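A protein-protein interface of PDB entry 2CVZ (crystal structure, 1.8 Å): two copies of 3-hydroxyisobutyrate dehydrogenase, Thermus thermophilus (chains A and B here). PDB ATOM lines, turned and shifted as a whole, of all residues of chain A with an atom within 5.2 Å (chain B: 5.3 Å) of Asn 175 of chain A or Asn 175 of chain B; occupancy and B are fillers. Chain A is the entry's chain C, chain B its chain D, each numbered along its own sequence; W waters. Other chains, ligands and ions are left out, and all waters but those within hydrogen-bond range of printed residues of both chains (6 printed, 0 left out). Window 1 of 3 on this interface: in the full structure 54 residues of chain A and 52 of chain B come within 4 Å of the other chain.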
ATOM      1  N   ALA A 170      26.908  18.549   8.277  1.00  0.00           N
ATOM      2  CA  ALA A 170      27.581  17.311   7.907  1.00  0.00           C
ATOM      3  C   ALA A 170      27.892  16.564   9.209  1.00  0.00           C
ATOM      4  O   ALA A 170      27.772  15.343   9.281  1.00  0.00           O
ATOM      5  CB  ALA A 170      28.870  17.606   7.145  1.00  0.00           C
ATOM      6  N   LEU A 171      28.281  17.300  10.246  1.00  0.00           N
ATOM      7  CA  LEU A 171      28.579  16.662  11.521  1.00  0.00           C
ATOM      8  C   LEU A 171      27.301  16.084  12.124  1.00  0.00           C
ATOM      9  O   LEU A 171      27.306  14.972  12.655  1.00  0.00           O
ATOM     10  CB  LEU A 171      29.223  17.651  12.491  1.00  0.00           C
ATOM     11  CG  LEU A 171      30.580  18.220  12.067  1.00  0.00           C
ATOM     12  CD1 LEU A 171      31.189  18.979  13.238  1.00  0.00           C
ATOM     13  CD2 LEU A 171      31.511  17.098  11.629  1.00  0.00           C
ATOM     14  N   LEU A 172      26.207  16.837  12.041  1.00  0.00           N
ATOM     15  CA  LEU A 172      24.929  16.358  12.559  1.00  0.00           C
ATOM     16  C   LEU A 172      24.567  15.054  11.842  1.00  0.00           C
ATOM     17  O   LEU A 172      24.176  14.071  12.473  1.00  0.00           O
ATOM     18  CB  LEU A 172      23.837  17.415  12.330  1.00  0.00           C
ATOM     19  CG  LEU A 172      22.361  17.091  12.617  1.00  0.00           C
ATOM     20  CD1 LEU A 172      21.780  16.290  11.475  1.00  0.00           C
ATOM     21  CD2 LEU A 172      22.226  16.339  13.937  1.00  0.00           C
ATOM     22  N   ALA A 173      24.720  15.052  10.520  1.00  0.00           N
ATOM     23  CA  ALA A 173      24.403  13.875   9.712  1.00  0.00           C
ATOM     24  C   ALA A 173      25.191  12.647  10.165  1.00  0.00           C
ATOM     25  O   ALA A 173      24.626  11.571  10.371  1.00  0.00           O
ATOM     26  CB  ALA A 173      24.683  14.166   8.233  1.00  0.00           C
ATOM     27  N   VAL A 174      26.498  12.804  10.316  1.00  0.00           N
ATOM     28  CA  VAL A 174      27.336  11.699  10.759  1.00  0.00           C
ATOM     29  C   VAL A 174      26.948  11.236  12.159  1.00  0.00           C
ATOM     30  O   VAL A 174      26.796  10.041  12.414  1.00  0.00           O
ATOM     31  CB  VAL A 174      28.823  12.103  10.766  1.00  0.00           C
ATOM     32  CG1 VAL A 174      29.635  11.063  11.510  1.00  0.00           C
ATOM     33  CG2 VAL A 174      29.329  12.237   9.342  1.00  0.00           C
ATOM     34  N   ASN A 175      26.791  12.186  13.073  1.00  0.00           N
ATOM     35  CA  ASN A 175      26.436  11.846  14.444  1.00  0.00           C
ATOM     36  C   ASN A 175      25.135  11.060  14.507  1.00  0.00           C
ATOM     37  O   ASN A 175      25.045  10.038  15.188  1.00  0.00           O
ATOM     38  CB  ASN A 175      26.303  13.115  15.288  1.00  0.00           C
ATOM     39  CG  ASN A 175      27.606  13.886  15.396  1.00  0.00           C
ATOM     40  OD1 ASN A 175      28.673  13.389  15.026  1.00  0.00           O
ATOM     41  ND2 ASN A 175      27.528  15.104  15.916  1.00  0.00           N
ATOM     42  N   LEU A 176      24.131  11.547  13.785  1.00  0.00           N
ATOM     43  CA  LEU A 176      22.815  10.925  13.762  1.00  0.00           C
ATOM     44  C   LEU A 176      22.810   9.534  13.143  1.00  0.00           C
ATOM     45  O   LEU A 176      22.215   8.607  13.690  1.00  0.00           O
ATOM     46  CB  LEU A 176      21.839  11.833  13.008  1.00  0.00           C
ATOM     47  CG  LEU A 176      20.417  11.323  12.758  1.00  0.00           C
ATOM     48  CD1 LEU A 176      19.708  11.049  14.081  1.00  0.00           C
ATOM     49  CD2 LEU A 176      19.653  12.368  11.959  1.00  0.00           C
ATOM     50  N   TRP A 177      23.475   9.384  12.003  1.00  0.00           N
ATOM     51  CA  TRP A 177      23.512   8.094  11.328  1.00  0.00           C
ATOM     52  C   TRP A 177      24.297   7.041  12.101  1.00  0.00           C
ATOM     53  O   TRP A 177      23.839   5.911  12.247  1.00  0.00           O
ATOM     54  CB  TRP A 177      24.088   8.253   9.918  1.00  0.00           C
ATOM     55  CG  TRP A 177      24.085   6.974   9.133  1.00  0.00           C
ATOM     56  CD1 TRP A 177      25.040   5.997   9.150  1.00  0.00           C
ATOM     57  CD2 TRP A 177      23.062   6.518   8.241  1.00  0.00           C
ATOM     58  NE1 TRP A 177      24.677   4.965   8.324  1.00  0.00           N
ATOM     59  CE2 TRP A 177      23.467   5.257   7.752  1.00  0.00           C
ATOM     60  CE3 TRP A 177      21.841   7.054   7.807  1.00  0.00           C
ATOM     61  CZ2 TRP A 177      22.694   4.519   6.850  1.00  0.00           C
ATOM     62  CZ3 TRP A 177      21.071   6.318   6.908  1.00  0.00           C
ATOM     63  CH2 TRP A 177      21.504   5.063   6.440  1.00  0.00           C
ATOM     64  N   ALA A 178      25.475   7.409  12.601  1.00  0.00           N
ATOM     65  CA  ALA A 178      26.294   6.466  13.355  1.00  0.00           C
ATOM     66  C   ALA A 178      25.546   5.991  14.592  1.00  0.00           C
ATOM     67  O   ALA A 178      25.597   4.812  14.947  1.00  0.00           O
ATOM     68  CB  ALA A 178      27.619   7.114  13.757  1.00  0.00           C
ATOM     69  N   ALA A 179      24.859   6.913  15.258  1.00  0.00           N
ATOM     70  CA  ALA A 179      24.093   6.551  16.443  1.00  0.00           C
ATOM     71  C   ALA A 179      23.049   5.520  16.016  1.00  0.00           C
ATOM     72  O   ALA A 179      22.788   4.551  16.729  1.00  0.00           O
ATOM     73  CB  ALA A 179      23.420   7.778  17.026  1.00  0.00           C
ATOM     74  N   GLY A 180      22.466   5.737  14.840  1.00  0.00           N
ATOM     75  CA  GLY A 180      21.471   4.821  14.312  1.00  0.00           C
ATOM     76  C   GLY A 180      22.046   3.433  14.093  1.00  0.00           C
ATOM     77  O   GLY A 180      21.441   2.433  14.492  1.00  0.00           O
ATOM     78  N   GLY A 205      30.023   9.462  24.229  1.00  0.00           N
ATOM     79  CA  GLY A 205      29.450   9.333  22.897  1.00  0.00           C
ATOM     80  C   GLY A 205      28.255  10.224  22.608  1.00  0.00           C
ATOM     81  O   GLY A 205      27.726  10.210  21.498  1.00  0.00           O
ATOM     82  N   ARG A 206      27.834  11.014  23.589  1.00  0.00           N
ATOM     83  CA  ARG A 206      26.678  11.881  23.399  1.00  0.00           C
ATOM     84  C   ARG A 206      26.863  12.964  22.344  1.00  0.00           C
ATOM     85  O   ARG A 206      27.965  13.457  22.114  1.00  0.00           O
ATOM     86  CB  ARG A 206      26.280  12.544  24.723  1.00  0.00           C
ATOM     87  CG  ARG A 206      27.291  13.536  25.278  1.00  0.00           C
ATOM     88  CD  ARG A 206      26.703  14.275  26.484  1.00  0.00           C
ATOM     89  NE  ARG A 206      27.629  15.233  27.089  1.00  0.00           N
ATOM     90  CZ  ARG A 206      28.677  14.902  27.838  1.00  0.00           C
ATOM     91  NH1 ARG A 206      28.951  13.626  28.086  1.00  0.00           N
ATOM     92  NH2 ARG A 206      29.452  15.850  28.350  1.00  0.00           N
ATOM     93  N   SER A 207      25.757  13.325  21.706  1.00  0.00           N
ATOM     94  CA  SER A 207      25.751  14.376  20.702  1.00  0.00           C
ATOM     95  C   SER A 207      24.352  14.967  20.713  1.00  0.00           C
ATOM     96  O   SER A 207      23.444  14.401  21.320  1.00  0.00           O
ATOM     97  CB  SER A 207      26.055  13.805  19.315  1.00  0.00           C
ATOM     98  OG  SER A 207      25.035  12.911  18.900  1.00  0.00           O
ATOM     99  N   ALA A 209      22.388  14.855  18.487  1.00  0.00           N
ATOM    100  CA  ALA A 209      21.556  13.843  17.843  1.00  0.00           C
ATOM    101  C   ALA A 209      21.002  12.825  18.840  1.00  0.00           C
ATOM    102  O   ALA A 209      19.816  12.495  18.799  1.00  0.00           O
ATOM    103  CB  ALA A 209      22.352  13.120  16.753  1.00  0.00           C
ATOM    104  N   ALA B 170      32.463   3.876  20.327  1.00  0.00           N
ATOM    105  CA  ALA B 170      32.493   3.879  18.868  1.00  0.00           C
ATOM    106  C   ALA B 170      31.883   5.191  18.379  1.00  0.00           C
ATOM    107  O   ALA B 170      32.371   5.787  17.421  1.00  0.00           O
ATOM    108  CB  ALA B 170      31.706   2.685  18.310  1.00  0.00           C
ATOM    109  N   LEU B 171      30.817   5.641  19.044  1.00  0.00           N
ATOM    110  CA  LEU B 171      30.161   6.891  18.670  1.00  0.00           C
ATOM    111  C   LEU B 171      31.086   8.065  18.967  1.00  0.00           C
ATOM    112  O   LEU B 171      31.157   9.027  18.196  1.00  0.00           O
ATOM    113  CB  LEU B 171      28.836   7.053  19.424  1.00  0.00           C
ATOM    114  CG  LEU B 171      27.752   6.027  19.070  1.00  0.00           C
ATOM    115  CD1 LEU B 171      26.447   6.399  19.769  1.00  0.00           C
ATOM    116  CD2 LEU B 171      27.543   5.991  17.551  1.00  0.00           C
ATOM    117  N   LEU B 172      31.793   7.988  20.089  1.00  0.00           N
ATOM    118  CA  LEU B 172      32.743   9.036  20.442  1.00  0.00           C
ATOM    119  C   LEU B 172      33.776   9.113  19.322  1.00  0.00           C
ATOM    120  O   LEU B 172      34.126  10.194  18.855  1.00  0.00           O
ATOM    121  CB  LEU B 172      33.455   8.705  21.754  1.00  0.00           C
ATOM    122  CG  LEU B 172      34.700   9.549  22.053  1.00  0.00           C
ATOM    123  CD1 LEU B 172      34.325  11.022  22.107  1.00  0.00           C
ATOM    124  CD2 LEU B 172      35.320   9.096  23.369  1.00  0.00           C
ATOM    125  N   ALA B 173      34.253   7.951  18.891  1.00  0.00           N
ATOM    126  CA  ALA B 173      35.252   7.896  17.830  1.00  0.00           C
ATOM    127  C   ALA B 173      34.757   8.540  16.537  1.00  0.00           C
ATOM    128  O   ALA B 173      35.436   9.386  15.958  1.00  0.00           O
ATOM    129  CB  ALA B 173      35.664   6.451  17.581  1.00  0.00           C
ATOM    130  N   VAL B 174      33.573   8.150  16.079  1.00  0.00           N
ATOM    131  CA  VAL B 174      33.032   8.717  14.846  1.00  0.00           C
ATOM    132  C   VAL B 174      32.843  10.224  14.942  1.00  0.00           C
ATOM    133  O   VAL B 174      33.253  10.971  14.052  1.00  0.00           O
ATOM    134  CB  VAL B 174      31.671   8.089  14.489  1.00  0.00           C
ATOM    135  CG1 VAL B 174      31.088   8.787  13.265  1.00  0.00           C
ATOM    136  CG2 VAL B 174      31.844   6.618  14.203  1.00  0.00           C
ATOM    137  N   ASN B 175      32.210  10.669  16.023  1.00  0.00           N
ATOM    138  CA  ASN B 175      31.955  12.092  16.221  1.00  0.00           C
ATOM    139  C   ASN B 175      33.239  12.913  16.201  1.00  0.00           C
ATOM    140  O   ASN B 175      33.303  13.971  15.579  1.00  0.00           O
ATOM    141  CB  ASN B 175      31.243  12.327  17.552  1.00  0.00           C
ATOM    142  CG  ASN B 175      29.896  11.643  17.628  1.00  0.00           C
ATOM    143  OD1 ASN B 175      29.425  11.050  16.651  1.00  0.00           O
ATOM    144  ND2 ASN B 175      29.262  11.726  18.794  1.00  0.00           N
ATOM    145  N   LEU B 176      34.256  12.415  16.894  1.00  0.00           N
ATOM    146  CA  LEU B 176      35.546  13.090  16.990  1.00  0.00           C
ATOM    147  C   LEU B 176      36.277  13.176  15.650  1.00  0.00           C
ATOM    148  O   LEU B 176      36.793  14.233  15.284  1.00  0.00           O
ATOM    149  CB  LEU B 176      36.430  12.363  18.012  1.00  0.00           C
ATOM    150  CG  LEU B 176      37.854  12.881  18.220  1.00  0.00           C
ATOM    151  CD1 LEU B 176      37.811  14.300  18.764  1.00  0.00           C
ATOM    152  CD2 LEU B 176      38.593  11.965  19.185  1.00  0.00           C
ATOM    153  N   TRP B 177      36.331  12.065  14.924  1.00  0.00           N
ATOM    154  CA  TRP B 177      37.016  12.051  13.637  1.00  0.00           C
ATOM    155  C   TRP B 177      36.310  12.905  12.587  1.00  0.00           C
ATOM    156  O   TRP B 177      36.960  13.646  11.848  1.00  0.00           O
ATOM    157  CB  TRP B 177      37.171  10.613  13.126  1.00  0.00           C
ATOM    158  CG  TRP B 177      37.953  10.524  11.851  1.00  0.00           C
ATOM    159  CD1 TRP B 177      37.490  10.739  10.580  1.00  0.00           C
ATOM    160  CD2 TRP B 177      39.351  10.255  11.727  1.00  0.00           C
ATOM    161  NE1 TRP B 177      38.519  10.622   9.676  1.00  0.00           N
ATOM    162  CE2 TRP B 177      39.672  10.326  10.353  1.00  0.00           C
ATOM    163  CE3 TRP B 177      40.369   9.963  12.648  1.00  0.00           C
ATOM    164  CZ2 TRP B 177      40.971  10.115   9.875  1.00  0.00           C
ATOM    165  CZ3 TRP B 177      41.661   9.754  12.172  1.00  0.00           C
ATOM    166  CH2 TRP B 177      41.949   9.833  10.797  1.00  0.00           C
ATOM    167  N   ALA B 178      34.986  12.798  12.513  1.00  0.00           N
ATOM    168  CA  ALA B 178      34.226  13.585  11.549  1.00  0.00           C
ATOM    169  C   ALA B 178      34.438  15.066  11.848  1.00  0.00           C
ATOM    170  O   ALA B 178      34.650  15.865  10.937  1.00  0.00           O
ATOM    171  CB  ALA B 178      32.746  13.240  11.625  1.00  0.00           C
ATOM    172  N   ALA B 179      34.372  15.432  13.126  1.00  0.00           N
ATOM    173  CA  ALA B 179      34.581  16.822  13.516  1.00  0.00           C
ATOM    174  C   ALA B 179      35.956  17.272  13.031  1.00  0.00           C
ATOM    175  O   ALA B 179      36.122  18.401  12.565  1.00  0.00           O
ATOM    176  CB  ALA B 179      34.479  16.971  15.035  1.00  0.00           C
ATOM    177  N   GLY B 180      36.940  16.381  13.138  1.00  0.00           N
ATOM    178  CA  GLY B 180      38.286  16.699  12.690  1.00  0.00           C
ATOM    179  C   GLY B 180      38.342  17.001  11.201  1.00  0.00           C
ATOM    180  O   GLY B 180      38.930  18.003  10.785  1.00  0.00           O
ATOM    181  N   SER B 204      23.320  22.308  15.858  1.00  0.00           N
ATOM    182  CA  SER B 204      22.909  20.911  15.747  1.00  0.00           C
ATOM    183  C   SER B 204      24.032  19.883  15.604  1.00  0.00           C
ATOM    184  O   SER B 204      23.836  18.709  15.920  1.00  0.00           O
ATOM    185  CB  SER B 204      21.947  20.756  14.569  1.00  0.00           C
ATOM    186  OG  SER B 204      22.590  21.095  13.351  1.00  0.00           O
ATOM    187  N   GLY B 205      25.196  20.317  15.133  1.00  0.00           N
ATOM    188  CA  GLY B 205      26.305  19.392  14.947  1.00  0.00           C
ATOM    189  C   GLY B 205      27.139  19.112  16.185  1.00  0.00           C
ATOM    190  O   GLY B 205      28.065  18.301  16.140  1.00  0.00           O
ATOM    191  N   ARG B 206      26.815  19.768  17.292  1.00  0.00           N
ATOM    192  CA  ARG B 206      27.567  19.586  18.530  1.00  0.00           C
ATOM    193  C   ARG B 206      27.546  18.172  19.102  1.00  0.00           C
ATOM    194  O   ARG B 206      26.592  17.414  18.909  1.00  0.00           O
ATOM    195  CB  ARG B 206      27.064  20.555  19.606  1.00  0.00           C
ATOM    196  CG  ARG B 206      25.634  20.306  20.076  1.00  0.00           C
ATOM    197  CD  ARG B 206      25.300  21.211  21.255  1.00  0.00           C
ATOM    198  NE  ARG B 206      23.964  20.979  21.802  1.00  0.00           N
ATOM    199  CZ  ARG B 206      22.829  21.342  21.211  1.00  0.00           C
ATOM    200  NH1 ARG B 206      22.847  21.960  20.036  1.00  0.00           N
ATOM    201  NH2 ARG B 206      21.667  21.096  21.807  1.00  0.00           N
ATOM    202  N   SER B 207      28.619  17.837  19.813  1.00  0.00           N
ATOM    203  CA  SER B 207      28.765  16.546  20.469  1.00  0.00           C
ATOM    204  C   SER B 207      29.746  16.748  21.616  1.00  0.00           C
ATOM    205  O   SER B 207      30.381  17.800  21.719  1.00  0.00           O
ATOM    206  CB  SER B 207      29.330  15.502  19.504  1.00  0.00           C
ATOM    207  OG  SER B 207      30.639  15.856  19.091  1.00  0.00           O
ATOM    208  N   ALA B 209      32.488  15.542  21.848  1.00  0.00           N
ATOM    209  CA  ALA B 209      33.794  15.710  21.217  1.00  0.00           C
ATOM    210  C   ALA B 209      34.113  17.172  20.885  1.00  0.00           C
ATOM    211  O   ALA B 209      35.206  17.655  21.173  1.00  0.00           O
ATOM    212  CB  ALA B 209      33.875  14.854  19.947  1.00  0.00           C
HETATM  213  O   HOH W   1      30.949  15.120  14.597  1.00  0.00           O
HETATM  214  O   HOH W   2      26.230  10.579  19.253  1.00  0.00           O
HETATM  215  O   HOH W   3      30.630  12.629  21.411  1.00  0.00           O
HETATM  216  O   HOH W   4      24.987  16.423  16.859  1.00  0.00           O
HETATM  217  O   HOH W   5      27.138   9.319  17.025  1.00  0.00           O
HETATM  218  O   HOH W   6      30.184  16.712  16.540  1.00  0.00           O
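OD1 of Asn 175 of chain B lies close to OD1 of Asn 175 of chain A (2.9 Å). The side-chain amide nitrogen of Asn 175 of chain A is in hydrogen-bond range of the backbone carbonyl oxygen of Gly 205 of chain B. The backbone carbonyl oxygen (O) of Gly 205 of chain A is in hydrogen-bond range of the side-chain amide nitrogen (ND2) of Asn 175 of chain B.
O of Leu 171 of chain A lies close to OD1 of Asn 175 of chain A, at 3.2 Å. The side-chain hydroxyl (OG) of Ser 207 of chain A lies close to the backbone NH (N) of Ala 209 of chain A (3.3 Å). The backbone carbonyl oxygen (O) of Leu 171 of chain B lies close to the side-chain amide oxygen (OD1) of Asn 175 of chain B (3.1 Å). The side-chain hydroxyl (OG) of Ser 207 of chain B lies close to the backbone NH (N) of Ala 209 of chain B, at 3.3 Å.
Among the printed residues, merely in contact across the chains: Leu 171 of chain A with Ala 178 of chain B, Leu 171 of chain A with Ala 179 of chain B, Leu 171 of chain A with Gly 205 of chain B, Leu 172 of chain A with Ser 204 of chain B, Leu 172 of chain A with Gly 205 of chain B, Val 174 of chain A with Val 174 of chain B, Val 174 of chain A with Ala 178 of chain B, Asn 175 of chain A with Arg 206 of chain B, Ala 178 of chain A with Leu 171 of chain B, Ala 178 of chain A with Val 174 of chain B, Ala 179 of chain A with Leu 171 of chain B, Gly 205 of chain A with Leu 171 of chain B, Gly 205 of chain A with Leu 172 of chain B, Arg 206 of chain A with Asn 175 of chain B, Arg 206 of chain A with Ser 207 of chain B, Ser 207 of chain A with Asn 175 of chain B, Ser 207 of chain A with Arg 206 of chain B and Ser 207 of chain A with Ser 207 of chain B.
Of chain B, only Asn 175 (2.9 Å), Gly 205 (3.2 Å) and Arg 206 (3.9 Å) come within 4 Å of Asn 175 of chain A. Asn 175 of chain B touches just these residues of chain A: Asn 175, Gly 205, Arg 206 and Ser 207. Printed residues of chain B within 4 Å of Val 174 of chain A: Val 174 (3.2 Å) and Ala 178 (3.8 Å). Printed residues of chain A within 4 Å of Val 174 of chain B: Val 174 and Ala 178. Printed residues of chain B within 4 Å of Ala 179 of chain A: Leu 171. Ala 173 of chain B touches none of the printed residues of chain A. Ala 170 of chain A touches none of the printed residues of chain B.
Hydrophobic or aromatic side chains of chain A within 4 Å of the printed part of chain B: Leu 171, Leu 172, Val 174 and Ala 178. Along chain A the printed residues that touch a printed residue of chain B span positions 171 to 207. Of the 16 printed residues of chain B, 10 touch a printed residue of chain A. Hydrophobic or aromatic side chains of chain B within 4 Å of the printed part of chain A: Leu 171, Val 174 and Ala 178. Along chain B the printed residues that touch a printed residue of chain A span positions 171 to 207.
Leu 171 of chain A touches Ala 178 of chain B, and with the chains exchanged Ala 178 of chain A touches Leu 171 of chain B. Leu 171 of chain A touches Ala 179 of chain B, and with the chains exchanged Ala 179 of chain A touches Leu 171 of chain B. Leu 171 of chain A touches Gly 205 of chain B, and with the chains exchanged Gly 205 of chain A touches Leu 171 of chain B. Asn 175 of chain A touches Arg 206 of chain B, and with the chains exchanged Arg 206 of chain A touches Asn 175 of chain B. 15 positions are printed for both chains.
Water W2 lies within hydrogen-bond range of the side-chain hydroxyl (OG) of Ser 207 of chain A (2.6 Å), the backbone carbonyl oxygen (O) of Gly 205 of chain A (2.7 Å) and the side-chain amide nitrogen (ND2) of Asn 175 of chain B (3.3 Å). Water W6 lies within hydrogen-bond range of O of Gly 205 of chain B, OG of Ser 207 of chain B and ND2 of Asn 175 of chain A. Water W4 lies within hydrogen-bond range of O of Ser 204 of chain B (2.7 Å), O of Arg 206 of chain B (2.8 Å), ND2 of Asn 175 of chain A (3.0 Å) and N of Ala 209 of chain A (3.4 Å). Water W1 lies within hydrogen-bond range of the backbone carbonyl oxygen (O) of Asn 175 of chain B and the side-chain amide oxygen (OD1) of Asn 175 of chain A. Water W5 lies within hydrogen-bond range of the backbone carbonyl oxygen of Asn 175 of chain A (2.9 Å) and the side-chain amide oxygen of Asn 175 of chain B (2.9 Å). Water W3 lies within hydrogen-bond range of O of Arg 206 of chain A (2.9 Å), ND2 of Asn 175 of chain B (3.1 Å) and N of Ala 209 of chain B (3.5 Å).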
